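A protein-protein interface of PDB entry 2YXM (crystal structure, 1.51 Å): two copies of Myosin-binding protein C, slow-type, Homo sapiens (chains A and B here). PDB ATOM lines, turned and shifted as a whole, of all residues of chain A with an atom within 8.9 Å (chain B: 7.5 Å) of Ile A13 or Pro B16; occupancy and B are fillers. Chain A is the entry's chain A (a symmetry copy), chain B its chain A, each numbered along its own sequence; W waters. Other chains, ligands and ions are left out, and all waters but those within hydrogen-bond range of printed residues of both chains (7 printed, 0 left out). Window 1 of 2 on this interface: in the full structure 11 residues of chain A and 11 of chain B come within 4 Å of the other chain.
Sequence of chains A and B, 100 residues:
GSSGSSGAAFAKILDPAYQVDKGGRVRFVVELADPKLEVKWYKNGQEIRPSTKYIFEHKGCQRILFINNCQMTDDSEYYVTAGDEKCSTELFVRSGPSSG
Hydrophobic or aromatic side chains of chain A that line the printed part of chain B: Ile A13 and Pro A16. Hydrophobic or aromatic side chains of chain B within 4 Å of the printed part of chain A: Ile B13, Pro B16 and Phe B92. Along chain B the printed residues that touch a printed residue of chain A span positions 13 to 92. Among the printed residues, 4 pairs touch across the chains.
Of the printed residues of chain B, Ile A13 touches Pro B16. Of the printed residues of chain A, Ile B13 touches Pro A16. Of the printed residues of chain B, Glu A85 touches Glu B90 (2.5 Å) and Phe B92 (3.9 Å). Of the printed residues of chain B, Pro A16 touches Ile B13. Tyr A18 touches none of the printed residues of chain B.
Ile A13 touches Pro B16 (CD1 to CG, 3.3 Å). Pro A16 touches Ile B13 (CG to CD1, 3.3 Å). CZ of Phe B92 touches OE2 of Glu A85 (3.9 Å).
The side-chain hydroxyl (OG1) of Thr B89 sits at hydrogen-bond distance from the backbone carbonyl oxygen (O) of Pro B16 (3.2 Å). The backbone NH of Glu B90 sits at hydrogen-bond distance from the backbone carbonyl oxygen of Pro B16 (3.2 Å). The backbone NH (N) of Tyr B18 is in hydrogen-bond range of the backbone carbonyl oxygen (O) of Glu B90 (2.9 Å). The backbone carbonyl oxygen (O) of Tyr B18 lies within hydrogen-bond range of the backbone NH (N) of Phe B92 (2.8 Å). OE1 of Glu A85 lies within hydrogen-bond range of N of Ala A9, 2.9 Å away. O of Pro A16 is in hydrogen-bond range of OG1 of Thr A89, at 3.2 Å.
OE2 of Glu A85 lies close to OE1 of Glu B90 (2.5 Å).
Water W3 lies within hydrogen-bond range of the backbone carbonyl oxygen (O) of Lys A86 and the side-chain carboxylate (OE2) of Glu B90. Water W7 bridges OE2 of Glu B90 (2.8 Å) and N of Lys A86 (3.1 Å). Water W2 lies within hydrogen-bond range of N of Ser B88 (3.0 Å) and OG of Ser A88 (3.4 Å). Water W5 bridges the backbone NH of Ser A88 (3.0 Å) and the side-chain hydroxyl of Ser B88 (3.4 Å). Water W6 bridges the side-chain hydroxyl of Ser B88 (3.0 Å) and the backbone carbonyl oxygen of Lys A86 (3.5 Å). Water W4 lies within hydrogen-bond range of O of Lys A86 (3.0 Å) and OG of Ser B88 (3.5 Å).
Ile A13 touches Pro B16, and with the chains exchanged Pro A16 touches Ile B13.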
ATOM      1  N   ALA A   9     -28.188   2.401  13.657  1.00  0.00           N
ATOM      2  CA  ALA A   9     -27.176   3.034  12.819  1.00  0.00           C
ATOM      3  C   ALA A   9     -26.640   2.173  11.680  1.00  0.00           C
ATOM      4  O   ALA A   9     -26.028   2.693  10.748  1.00  0.00           O
ATOM      5  CB  ALA A   9     -26.014   3.491  13.694  1.00  0.00           C
ATOM      6  N   PHE A  10     -26.868   0.867  11.748  1.00  0.00           N
ATOM      7  CA  PHE A  10     -26.367  -0.040  10.721  1.00  0.00           C
ATOM      8  C   PHE A  10     -27.399  -0.457   9.687  1.00  0.00           C
ATOM      9  O   PHE A  10     -28.385  -1.115  10.021  1.00  0.00           O
ATOM     10  CB  PHE A  10     -25.807  -1.318  11.363  1.00  0.00           C
ATOM     11  CG  PHE A  10     -24.524  -1.120  12.127  1.00  0.00           C
ATOM     12  CD1 PHE A  10     -23.323  -0.905  11.456  1.00  0.00           C
ATOM     13  CD2 PHE A  10     -24.516  -1.186  13.514  1.00  0.00           C
ATOM     14  CE1 PHE A  10     -22.130  -0.764  12.161  1.00  0.00           C
ATOM     15  CE2 PHE A  10     -23.328  -1.045  14.230  1.00  0.00           C
ATOM     16  CZ  PHE A  10     -22.134  -0.835  13.555  1.00  0.00           C
ATOM     17  N   ALA A  11     -27.171  -0.078   8.433  1.00  0.00           N
ATOM     18  CA  ALA A  11     -28.057  -0.479   7.348  1.00  0.00           C
ATOM     19  C   ALA A  11     -27.653  -1.911   6.998  1.00  0.00           C
ATOM     20  O   ALA A  11     -28.481  -2.734   6.618  1.00  0.00           O
ATOM     21  CB  ALA A  11     -27.875   0.438   6.137  1.00  0.00           C
ATOM     22  N   LYS A  12     -26.363  -2.203   7.141  1.00  0.00           N
ATOM     23  CA  LYS A  12     -25.839  -3.534   6.874  1.00  0.00           C
ATOM     24  C   LYS A  12     -24.739  -3.800   7.898  1.00  0.00           C
ATOM     25  O   LYS A  12     -23.851  -2.972   8.083  1.00  0.00           O
ATOM     26  CB  LYS A  12     -25.279  -3.603   5.449  1.00  0.00           C
ATOM     27  CG  LYS A  12     -24.994  -5.009   4.946  1.00  0.00           C
ATOM     28  CD  LYS A  12     -24.727  -5.015   3.439  1.00  0.00           C
ATOM     29  CE  LYS A  12     -25.960  -4.596   2.645  1.00  0.00           C
ATOM     30  NZ  LYS A  12     -25.737  -4.651   1.167  1.00  0.00           N
ATOM     31  N   ILE A  13     -24.814  -4.937   8.583  1.00  0.00           N
ATOM     32  CA  ILE A  13     -23.803  -5.272   9.580  1.00  0.00           C
ATOM     33  C   ILE A  13     -22.813  -6.295   9.039  1.00  0.00           C
ATOM     34  O   ILE A  13     -22.952  -6.778   7.917  1.00  0.00           O
ATOM     35  CB  ILE A  13     -24.429  -5.842  10.880  1.00  0.00           C
ATOM     36  CG1 ILE A  13     -25.210  -7.122  10.579  1.00  0.00           C
ATOM     37  CG2 ILE A  13     -25.322  -4.790  11.538  1.00  0.00           C
ATOM     38  CD1 ILE A  13     -25.476  -7.959  11.815  1.00  0.00           C
ATOM     39  N   LEU A  14     -21.805  -6.613   9.843  1.00  0.00           N
ATOM     40  CA  LEU A  14     -20.790  -7.587   9.452  1.00  0.00           C
ATOM     41  C   LEU A  14     -21.368  -8.994   9.377  1.00  0.00           C
ATOM     42  O   LEU A  14     -22.318  -9.318  10.089  1.00  0.00           O
ATOM     43  CB  LEU A  14     -19.652  -7.591  10.470  1.00  0.00           C
ATOM     44  CG  LEU A  14     -18.776  -6.344  10.564  1.00  0.00           C
ATOM     45  CD1 LEU A  14     -17.879  -6.455  11.791  1.00  0.00           C
ATOM     46  CD2 LEU A  14     -17.949  -6.203   9.291  1.00  0.00           C
ATOM     47  N   ASP A  15     -20.798  -9.827   8.508  1.00  0.00           N
ATOM     48  CA  ASP A  15     -21.239 -11.212   8.408  1.00  0.00           C
ATOM     49  C   ASP A  15     -20.796 -11.874   9.715  1.00  0.00           C
ATOM     50  O   ASP A  15     -19.914 -11.363  10.412  1.00  0.00           O
ATOM     51  CB  ASP A  15     -20.558 -11.949   7.247  1.00  0.00           C
ATOM     52  CG  ASP A  15     -20.911 -11.385   5.883  1.00  0.00           C
ATOM     53  OD1 ASP A  15     -21.941 -10.691   5.750  1.00  0.00           O
ATOM     54  OD2 ASP A  15     -20.154 -11.666   4.926  1.00  0.00           O
ATOM     55  N   PRO A  16     -21.389 -13.028  10.056  1.00  0.00           N
ATOM     56  CA  PRO A  16     -21.054 -13.759  11.282  1.00  0.00           C
ATOM     57  C   PRO A  16     -19.581 -14.157  11.392  1.00  0.00           C
ATOM     58  O   PRO A  16     -19.002 -14.143  12.479  1.00  0.00           O
ATOM     59  CB  PRO A  16     -21.967 -14.981  11.210  1.00  0.00           C
ATOM     60  CG  PRO A  16     -23.154 -14.472  10.485  1.00  0.00           C
ATOM     61  CD  PRO A  16     -22.539 -13.650   9.377  1.00  0.00           C
ATOM     62  N   TYR A  18     -15.722 -14.707   8.721  1.00  0.00           N
ATOM     63  CA  TYR A  18     -15.017 -14.616   7.446  1.00  0.00           C
ATOM     64  C   TYR A  18     -13.799 -15.524   7.548  1.00  0.00           C
ATOM     65  O   TYR A  18     -13.350 -15.843   8.645  1.00  0.00           O
ATOM     66  CB  TYR A  18     -14.507 -13.191   7.203  1.00  0.00           C
ATOM     67  CG  TYR A  18     -15.570 -12.127   7.108  1.00  0.00           C
ATOM     68  CD1 TYR A  18     -15.957 -11.610   5.873  1.00  0.00           C
ATOM     69  CD2 TYR A  18     -16.169 -11.608   8.257  1.00  0.00           C
ATOM     70  CE1 TYR A  18     -16.911 -10.598   5.780  1.00  0.00           C
ATOM     71  CE2 TYR A  18     -17.123 -10.597   8.176  1.00  0.00           C
ATOM     72  CZ  TYR A  18     -17.488 -10.097   6.935  1.00  0.00           C
ATOM     73  OH  TYR A  18     -18.414  -9.087   6.842  1.00  0.00           O
ATOM     74  N   PHE A  28     -13.655  -6.424   5.301  1.00  0.00           N
ATOM     75  CA  PHE A  28     -14.852  -6.345   6.139  1.00  0.00           C
ATOM     76  C   PHE A  28     -15.616  -5.116   5.670  1.00  0.00           C
ATOM     77  O   PHE A  28     -15.018  -4.062   5.452  1.00  0.00           O
ATOM     78  CB  PHE A  28     -14.516  -6.125   7.624  1.00  0.00           C
ATOM     79  CG  PHE A  28     -13.793  -7.265   8.287  1.00  0.00           C
ATOM     80  CD1 PHE A  28     -13.962  -8.579   7.867  1.00  0.00           C
ATOM     81  CD2 PHE A  28     -12.979  -7.016   9.386  1.00  0.00           C
ATOM     82  CE1 PHE A  28     -13.327  -9.623   8.532  1.00  0.00           C
ATOM     83  CE2 PHE A  28     -12.342  -8.054  10.059  1.00  0.00           C
ATOM     84  CZ  PHE A  28     -12.517  -9.359   9.629  1.00  0.00           C
ATOM     85  N   VAL A  29     -16.931  -5.234   5.532  1.00  0.00           N
ATOM     86  CA  VAL A  29     -17.731  -4.100   5.098  1.00  0.00           C
ATOM     87  C   VAL A  29     -19.026  -3.963   5.886  1.00  0.00           C
ATOM     88  O   VAL A  29     -19.698  -4.954   6.174  1.00  0.00           O
ATOM     89  CB  VAL A  29     -18.117  -4.218   3.602  1.00  0.00           C
ATOM     90  CG1 VAL A  29     -18.828  -2.949   3.140  1.00  0.00           C
ATOM     91  CG2 VAL A  29     -16.880  -4.486   2.761  1.00  0.00           C
ATOM     92  N   VAL A  30     -19.351  -2.732   6.265  1.00  0.00           N
ATOM     93  CA  VAL A  30     -20.614  -2.453   6.939  1.00  0.00           C
ATOM     94  C   VAL A  30     -21.184  -1.241   6.224  1.00  0.00           C
ATOM     95  O   VAL A  30     -20.455  -0.501   5.562  1.00  0.00           O
ATOM     96  CB  VAL A  30     -20.465  -2.133   8.455  1.00  0.00           C
ATOM     97  CG1 VAL A  30     -20.010  -3.377   9.203  1.00  0.00           C
ATOM     98  CG2 VAL A  30     -19.513  -0.968   8.670  1.00  0.00           C
ATOM     99  N   GLU A  31     -22.491  -1.050   6.324  1.00  0.00           N
ATOM    100  CA  GLU A  31     -23.121   0.093   5.687  1.00  0.00           C
ATOM    101  C   GLU A  31     -23.866   0.873   6.752  1.00  0.00           C
ATOM    102  O   GLU A  31     -24.629   0.303   7.533  1.00  0.00           O
ATOM    103  CB  GLU A  31     -24.096  -0.355   4.598  1.00  0.00           C
ATOM    104  CG  GLU A  31     -24.573   0.777   3.701  1.00  0.00           C
ATOM    105  CD  GLU A  31     -25.678   0.340   2.760  1.00  0.00           C
ATOM    106  OE1 GLU A  31     -25.571  -0.771   2.200  1.00  0.00           O
ATOM    107  OE2 GLU A  31     -26.644   1.111   2.575  1.00  0.00           O
ATOM    108  N   LEU A  32     -23.627   2.178   6.792  1.00  0.00           N
ATOM    109  CA  LEU A  32     -24.282   3.039   7.758  1.00  0.00           C
ATOM    110  C   LEU A  32     -25.469   3.709   7.092  1.00  0.00           C
ATOM    111  O   LEU A  32     -25.548   3.785   5.865  1.00  0.00           O
ATOM    112  CB  LEU A  32     -23.316   4.117   8.256  1.00  0.00           C
ATOM    113  CG  LEU A  32     -21.988   3.640   8.842  1.00  0.00           C
ATOM    114  CD1 LEU A  32     -21.218   4.838   9.377  1.00  0.00           C
ATOM    115  CD2 LEU A  32     -22.242   2.627   9.948  1.00  0.00           C
ATOM    116  N   TRP A  41     -13.053   0.609  14.625  1.00  0.00           N
ATOM    117  CA  TRP A  41     -12.880  -0.834  14.534  1.00  0.00           C
ATOM    118  C   TRP A  41     -12.036  -1.329  15.697  1.00  0.00           C
ATOM    119  O   TRP A  41     -11.118  -0.644  16.143  1.00  0.00           O
ATOM    120  CB  TRP A  41     -12.215  -1.213  13.210  1.00  0.00           C
ATOM    121  CG  TRP A  41     -13.035  -0.862  11.994  1.00  0.00           C
ATOM    122  CD1 TRP A  41     -13.158   0.366  11.414  1.00  0.00           C
ATOM    123  CD2 TRP A  41     -13.832  -1.758  11.211  1.00  0.00           C
ATOM    124  NE1 TRP A  41     -13.978   0.293  10.311  1.00  0.00           N
ATOM    125  CE2 TRP A  41     -14.406  -1.000  10.163  1.00  0.00           C
ATOM    126  CE3 TRP A  41     -14.118  -3.127  11.290  1.00  0.00           C
ATOM    127  CZ2 TRP A  41     -15.250  -1.568   9.200  1.00  0.00           C
ATOM    128  CZ3 TRP A  41     -14.958  -3.692  10.329  1.00  0.00           C
ATOM    129  CH2 TRP A  41     -15.512  -2.911   9.301  1.00  0.00           C
ATOM    130  N   ARG A  63     -18.387   1.489   5.016  1.00  0.00           N
ATOM    131  CA  ARG A  63     -17.195   1.629   5.847  1.00  0.00           C
ATOM    132  C   ARG A  63     -16.479   0.296   5.678  1.00  0.00           C
ATOM    133  O   ARG A  63     -17.028  -0.766   5.989  1.00  0.00           O
ATOM    134  CB  ARG A  63     -17.572   1.869   7.310  1.00  0.00           C
ATOM    135  CG  ARG A  63     -18.208   3.232   7.558  1.00  0.00           C
ATOM    136  CD  ARG A  63     -17.231   4.365   7.239  1.00  0.00           C
ATOM    137  NE  ARG A  63     -17.823   5.681   7.455  1.00  0.00           N
ATOM    138  CZ  ARG A  63     -18.765   6.214   6.684  1.00  0.00           C
ATOM    139  NH1 ARG A  63     -19.248   7.418   6.961  1.00  0.00           N
ATOM    140  NH2 ARG A  63     -19.219   5.549   5.631  1.00  0.00           N
ATOM    141  N   VAL A  80     -17.084  -3.447  15.203  1.00  0.00           N
ATOM    142  CA  VAL A  80     -17.070  -2.080  14.734  1.00  0.00           C
ATOM    143  C   VAL A  80     -18.222  -1.361  15.407  1.00  0.00           C
ATOM    144  O   VAL A  80     -19.296  -1.930  15.604  1.00  0.00           O
ATOM    145  CB  VAL A  80     -17.213  -2.030  13.189  1.00  0.00           C
ATOM    146  CG1 VAL A  80     -18.492  -2.733  12.755  1.00  0.00           C
ATOM    147  CG2 VAL A  80     -17.196  -0.594  12.706  1.00  0.00           C
ATOM    148  N   ALA A  82     -20.714   2.184  15.690  1.00  0.00           N
ATOM    149  CA  ALA A  82     -21.296   3.288  14.936  1.00  0.00           C
ATOM    150  C   ALA A  82     -22.424   3.823  15.806  1.00  0.00           C
ATOM    151  O   ALA A  82     -23.356   3.092  16.138  1.00  0.00           O
ATOM    152  CB  ALA A  82     -21.842   2.793  13.600  1.00  0.00           C
ATOM    153  N   GLU A  85     -24.301   1.802  18.686  1.00  0.00           N
ATOM    154  CA  GLU A  85     -24.353   0.376  18.385  1.00  0.00           C
ATOM    155  C   GLU A  85     -23.013  -0.217  17.973  1.00  0.00           C
ATOM    156  O   GLU A  85     -22.044   0.494  17.712  1.00  0.00           O
ATOM    157  CB  GLU A  85     -25.369   0.101  17.273  1.00  0.00           C
ATOM    158  CG  GLU A  85     -26.774   0.598  17.569  1.00  0.00           C
ATOM    159  CD  GLU A  85     -27.753   0.203  16.488  1.00  0.00           C
ATOM    160  OE1 GLU A  85     -27.360   0.215  15.304  1.00  0.00           O
ATOM    161  OE2 GLU A  85     -28.917  -0.111  16.820  1.00  0.00           O
ATOM    162  N   LYS A  86     -22.981  -1.541  17.916  1.00  0.00           N
ATOM    163  CA  LYS A  86     -21.785  -2.262  17.522  1.00  0.00           C
ATOM    164  C   LYS A  86     -22.181  -3.633  16.998  1.00  0.00           C
ATOM    165  O   LYS A  86     -23.202  -4.188  17.393  1.00  0.00           O
ATOM    166  CB  LYS A  86     -20.852  -2.460  18.717  1.00  0.00           C
ATOM    167  CG  LYS A  86     -21.432  -3.369  19.790  1.00  0.00           C
ATOM    168  CD  LYS A  86     -20.351  -4.077  20.599  1.00  0.00           C
ATOM    169  CE  LYS A  86     -19.469  -3.105  21.356  1.00  0.00           C
ATOM    170  NZ  LYS A  86     -18.482  -3.827  22.205  1.00  0.00           N
ATOM    171  N   CYS A  87     -21.382  -4.167  16.088  1.00  0.00           N
ATOM    172  CA  CYS A  87     -21.633  -5.504  15.579  1.00  0.00           C
ATOM    173  C   CYS A  87     -20.274  -6.171  15.520  1.00  0.00           C
ATOM    174  O   CYS A  87     -19.248  -5.492  15.450  1.00  0.00           O
ATOM    175  CB  CYS A  87     -22.317  -5.480  14.208  1.00  0.00           C
ATOM    176  SG  CYS A  87     -21.421  -4.682  12.884  1.00  0.00           S
ATOM    177  N   SER A  88     -20.260  -7.495  15.564  1.00  0.00           N
ATOM    178  CA  SER A  88     -19.006  -8.230  15.568  1.00  0.00           C
ATOM    179  C   SER A  88     -18.951  -9.367  14.573  1.00  0.00           C
ATOM    180  O   SER A  88     -19.954  -9.753  13.979  1.00  0.00           O
ATOM    181  CB  SER A  88     -18.753  -8.796  16.963  1.00  0.00           C
ATOM    182  OG  SER A  88     -19.785  -9.699  17.317  1.00  0.00           O
ATOM    183  N   THR A  89     -17.752  -9.906  14.413  1.00  0.00           N
ATOM    184  CA  THR A  89     -17.531 -11.021  13.516  1.00  0.00           C
ATOM    185  C   THR A  89     -16.306 -11.788  13.973  1.00  0.00           C
ATOM    186  O   THR A  89     -15.556 -11.332  14.834  1.00  0.00           O
ATOM    187  CB  THR A  89     -17.297 -10.548  12.070  1.00  0.00           C
ATOM    188  OG1 THR A  89     -17.338 -11.681  11.193  1.00  0.00           O
ATOM    189  CG2 THR A  89     -15.934  -9.862  11.937  1.00  0.00           C
ATOM    190  N   ILE B  13     -27.020 -18.112  13.771  1.00  0.00           N
ATOM    191  CA  ILE B  13     -26.903 -17.145  14.857  1.00  0.00           C
ATOM    192  C   ILE B  13     -28.139 -16.260  14.943  1.00  0.00           C
ATOM    193  O   ILE B  13     -29.051 -16.365  14.126  1.00  0.00           O
ATOM    194  CB  ILE B  13     -25.660 -16.230  14.695  1.00  0.00           C
ATOM    195  CG1 ILE B  13     -25.749 -15.437  13.391  1.00  0.00           C
ATOM    196  CG2 ILE B  13     -24.382 -17.067  14.750  1.00  0.00           C
ATOM    197  CD1 ILE B  13     -24.827 -14.233  13.365  1.00  0.00           C
ATOM    198  N   LEU B  14     -28.167 -15.393  15.950  1.00  0.00           N
ATOM    199  CA  LEU B  14     -29.288 -14.479  16.144  1.00  0.00           C
ATOM    200  C   LEU B  14     -29.347 -13.429  15.043  1.00  0.00           C
ATOM    201  O   LEU B  14     -28.320 -13.061  14.474  1.00  0.00           O
ATOM    202  CB  LEU B  14     -29.149 -13.760  17.484  1.00  0.00           C
ATOM    203  CG  LEU B  14     -29.285 -14.593  18.757  1.00  0.00           C
ATOM    204  CD1 LEU B  14     -28.869 -13.747  19.953  1.00  0.00           C
ATOM    205  CD2 LEU B  14     -30.724 -15.077  18.899  1.00  0.00           C
ATOM    206  N   ASP B  15     -30.553 -12.951  14.739  1.00  0.00           N
ATOM    207  CA  ASP B  15     -30.705 -11.898  13.743  1.00  0.00           C
ATOM    208  C   ASP B  15     -30.096 -10.647  14.380  1.00  0.00           C
ATOM    209  O   ASP B  15     -29.938 -10.576  15.603  1.00  0.00           O
ATOM    210  CB  ASP B  15     -32.181 -11.605  13.437  1.00  0.00           C
ATOM    211  CG  ASP B  15     -32.910 -12.775  12.804  1.00  0.00           C
ATOM    212  OD1 ASP B  15     -32.256 -13.680  12.243  1.00  0.00           O
ATOM    213  OD2 ASP B  15     -34.162 -12.771  12.848  1.00  0.00           O
ATOM    214  N   PRO B  16     -29.760  -9.637  13.563  1.00  0.00           N
ATOM    215  CA  PRO B  16     -29.168  -8.387  14.048  1.00  0.00           C
ATOM    216  C   PRO B  16     -30.026  -7.645  15.075  1.00  0.00           C
ATOM    217  O   PRO B  16     -29.506  -7.045  16.017  1.00  0.00           O
ATOM    218  CB  PRO B  16     -28.988  -7.576  12.768  1.00  0.00           C
ATOM    219  CG  PRO B  16     -28.750  -8.615  11.741  1.00  0.00           C
ATOM    220  CD  PRO B  16     -29.776  -9.668  12.090  1.00  0.00           C
ATOM    221  N   ALA B  17     -31.341  -7.689  14.885  1.00  0.00           N
ATOM    222  CA  ALA B  17     -32.265  -7.008  15.780  1.00  0.00           C
ATOM    223  C   ALA B  17     -33.666  -7.579  15.620  1.00  0.00           C
ATOM    224  O   ALA B  17     -34.005  -8.141  14.580  1.00  0.00           O
ATOM    225  CB  ALA B  17     -32.281  -5.512  15.473  1.00  0.00           C
ATOM    226  N   TYR B  18     -34.469  -7.422  16.667  1.00  0.00           N
ATOM    227  CA  TYR B  18     -35.851  -7.892  16.692  1.00  0.00           C
ATOM    228  C   TYR B  18     -36.689  -6.771  17.293  1.00  0.00           C
ATOM    229  O   TYR B  18     -36.165  -5.907  17.991  1.00  0.00           O
ATOM    230  CB  TYR B  18     -35.997  -9.113  17.607  1.00  0.00           C
ATOM    231  CG  TYR B  18     -35.206 -10.330  17.199  1.00  0.00           C
ATOM    232  CD1 TYR B  18     -35.826 -11.410  16.574  1.00  0.00           C
ATOM    233  CD2 TYR B  18     -33.840 -10.420  17.468  1.00  0.00           C
ATOM    234  CE1 TYR B  18     -35.110 -12.555  16.230  1.00  0.00           C
ATOM    235  CE2 TYR B  18     -33.114 -11.557  17.128  1.00  0.00           C
ATOM    236  CZ  TYR B  18     -33.755 -12.621  16.511  1.00  0.00           C
ATOM    237  OH  TYR B  18     -33.055 -13.757  16.187  1.00  0.00           O
ATOM    238  N   TYR B  78     -28.777  -8.247  23.817  1.00  0.00           N
ATOM    239  CA  TYR B  78     -28.772  -9.591  24.385  1.00  0.00           C
ATOM    240  C   TYR B  78     -27.752 -10.418  23.640  1.00  0.00           C
ATOM    241  O   TYR B  78     -27.452 -10.148  22.482  1.00  0.00           O
ATOM    242  CB  TYR B  78     -30.124 -10.283  24.180  1.00  0.00           C
ATOM    243  CG  TYR B  78     -31.272  -9.688  24.941  1.00  0.00           C
ATOM    244  CD1 TYR B  78     -31.653 -10.204  26.176  1.00  0.00           C
ATOM    245  CD2 TYR B  78     -31.965  -8.587  24.440  1.00  0.00           C
ATOM    246  CE1 TYR B  78     -32.694  -9.637  26.899  1.00  0.00           C
ATOM    247  CE2 TYR B  78     -33.006  -8.011  25.152  1.00  0.00           C
ATOM    248  CZ  TYR B  78     -33.364  -8.537  26.381  1.00  0.00           C
ATOM    249  OH  TYR B  78     -34.379  -7.955  27.099  1.00  0.00           O
ATOM    250  N   SER B  88     -24.792 -11.759  19.312  1.00  0.00           N
ATOM    251  CA  SER B  88     -25.687 -10.823  19.972  1.00  0.00           C
ATOM    252  C   SER B  88     -26.766 -10.259  19.076  1.00  0.00           C
ATOM    253  O   SER B  88     -26.743 -10.421  17.859  1.00  0.00           O
ATOM    254  CB  SER B  88     -24.876  -9.661  20.541  1.00  0.00           C
ATOM    255  OG  SER B  88     -24.218  -8.968  19.496  1.00  0.00           O
ATOM    256  N   THR B  89     -27.710  -9.577  19.707  1.00  0.00           N
ATOM    257  CA  THR B  89     -28.803  -8.950  18.993  1.00  0.00           C
ATOM    258  C   THR B  89     -29.334  -7.794  19.819  1.00  0.00           C
ATOM    259  O   THR B  89     -28.985  -7.636  20.987  1.00  0.00           O
ATOM    260  CB  THR B  89     -29.957  -9.937  18.741  1.00  0.00           C
ATOM    261  OG1 THR B  89     -30.887  -9.349  17.824  1.00  0.00           O
ATOM    262  CG2 THR B  89     -30.684 -10.267  20.048  1.00  0.00           C
ATOM    263  N   GLU B  90     -30.167  -6.976  19.194  1.00  0.00           N
ATOM    264  CA  GLU B  90     -30.783  -5.846  19.866  1.00  0.00           C
ATOM    265  C   GLU B  90     -32.288  -6.052  19.824  1.00  0.00           C
ATOM    266  O   GLU B  90     -32.831  -6.457  18.797  1.00  0.00           O
ATOM    267  CB  GLU B  90     -30.421  -4.538  19.155  1.00  0.00           C
ATOM    268  CG  GLU B  90     -28.998  -4.066  19.411  1.00  0.00           C
ATOM    269  CD  GLU B  90     -28.610  -2.879  18.553  1.00  0.00           C
ATOM    270  OE1 GLU B  90     -29.501  -2.071  18.214  1.00  0.00           O
ATOM    271  OE2 GLU B  90     -27.411  -2.748  18.227  1.00  0.00           O
ATOM    272  N   LEU B  91     -32.953  -5.802  20.947  1.00  0.00           N
ATOM    273  CA  LEU B  91     -34.404  -5.930  21.009  1.00  0.00           C
ATOM    274  C   LEU B  91     -35.001  -4.537  21.124  1.00  0.00           C
ATOM    275  O   LEU B  91     -34.675  -3.792  22.049  1.00  0.00           O
ATOM    276  CB  LEU B  91     -34.841  -6.756  22.225  1.00  0.00           C
ATOM    277  CG  LEU B  91     -36.363  -6.841  22.398  1.00  0.00           C
ATOM    278  CD1 LEU B  91     -36.981  -7.565  21.206  1.00  0.00           C
ATOM    279  CD2 LEU B  91     -36.691  -7.570  23.694  1.00  0.00           C
ATOM    280  N   PHE B  92     -35.870  -4.189  20.179  1.00  0.00           N
ATOM    281  CA  PHE B  92     -36.530  -2.889  20.192  1.00  0.00           C
ATOM    282  C   PHE B  92     -37.980  -3.078  20.614  1.00  0.00           C
ATOM    283  O   PHE B  92     -38.736  -3.784  19.953  1.00  0.00           O
ATOM    284  CB  PHE B  92     -36.498  -2.238  18.805  1.00  0.00           C
ATOM    285  CG  PHE B  92     -35.115  -1.997  18.268  1.00  0.00           C
ATOM    286  CD1 PHE B  92     -34.043  -1.763  19.126  1.00  0.00           C
ATOM    287  CD2 PHE B  92     -34.892  -1.963  16.896  1.00  0.00           C
ATOM    288  CE1 PHE B  92     -32.766  -1.497  18.624  1.00  0.00           C
ATOM    289  CE2 PHE B  92     -33.621  -1.697  16.380  1.00  0.00           C
ATOM    290  CZ  PHE B  92     -32.554  -1.464  17.246  1.00  0.00           C
HETATM  291  O   HOH W   1     -29.835   1.262  19.026  1.00  0.00           O
HETATM  292  O   HOH W   2     -22.815 -11.161  17.182  1.00  0.00           O
HETATM  293  O   HOH W   3     -25.662  -3.969  16.280  1.00  0.00           O
HETATM  294  O   HOH W   4     -23.942  -5.520  20.003  1.00  0.00           O
HETATM  295  O   HOH W   5     -22.923  -8.476  16.427  1.00  0.00           O
HETATM  296  O   HOH W   6     -21.954  -7.115  18.801  1.00  0.00           O
HETATM  297  O   HOH W   7     -25.089  -2.731  19.812  1.00  0.00           O
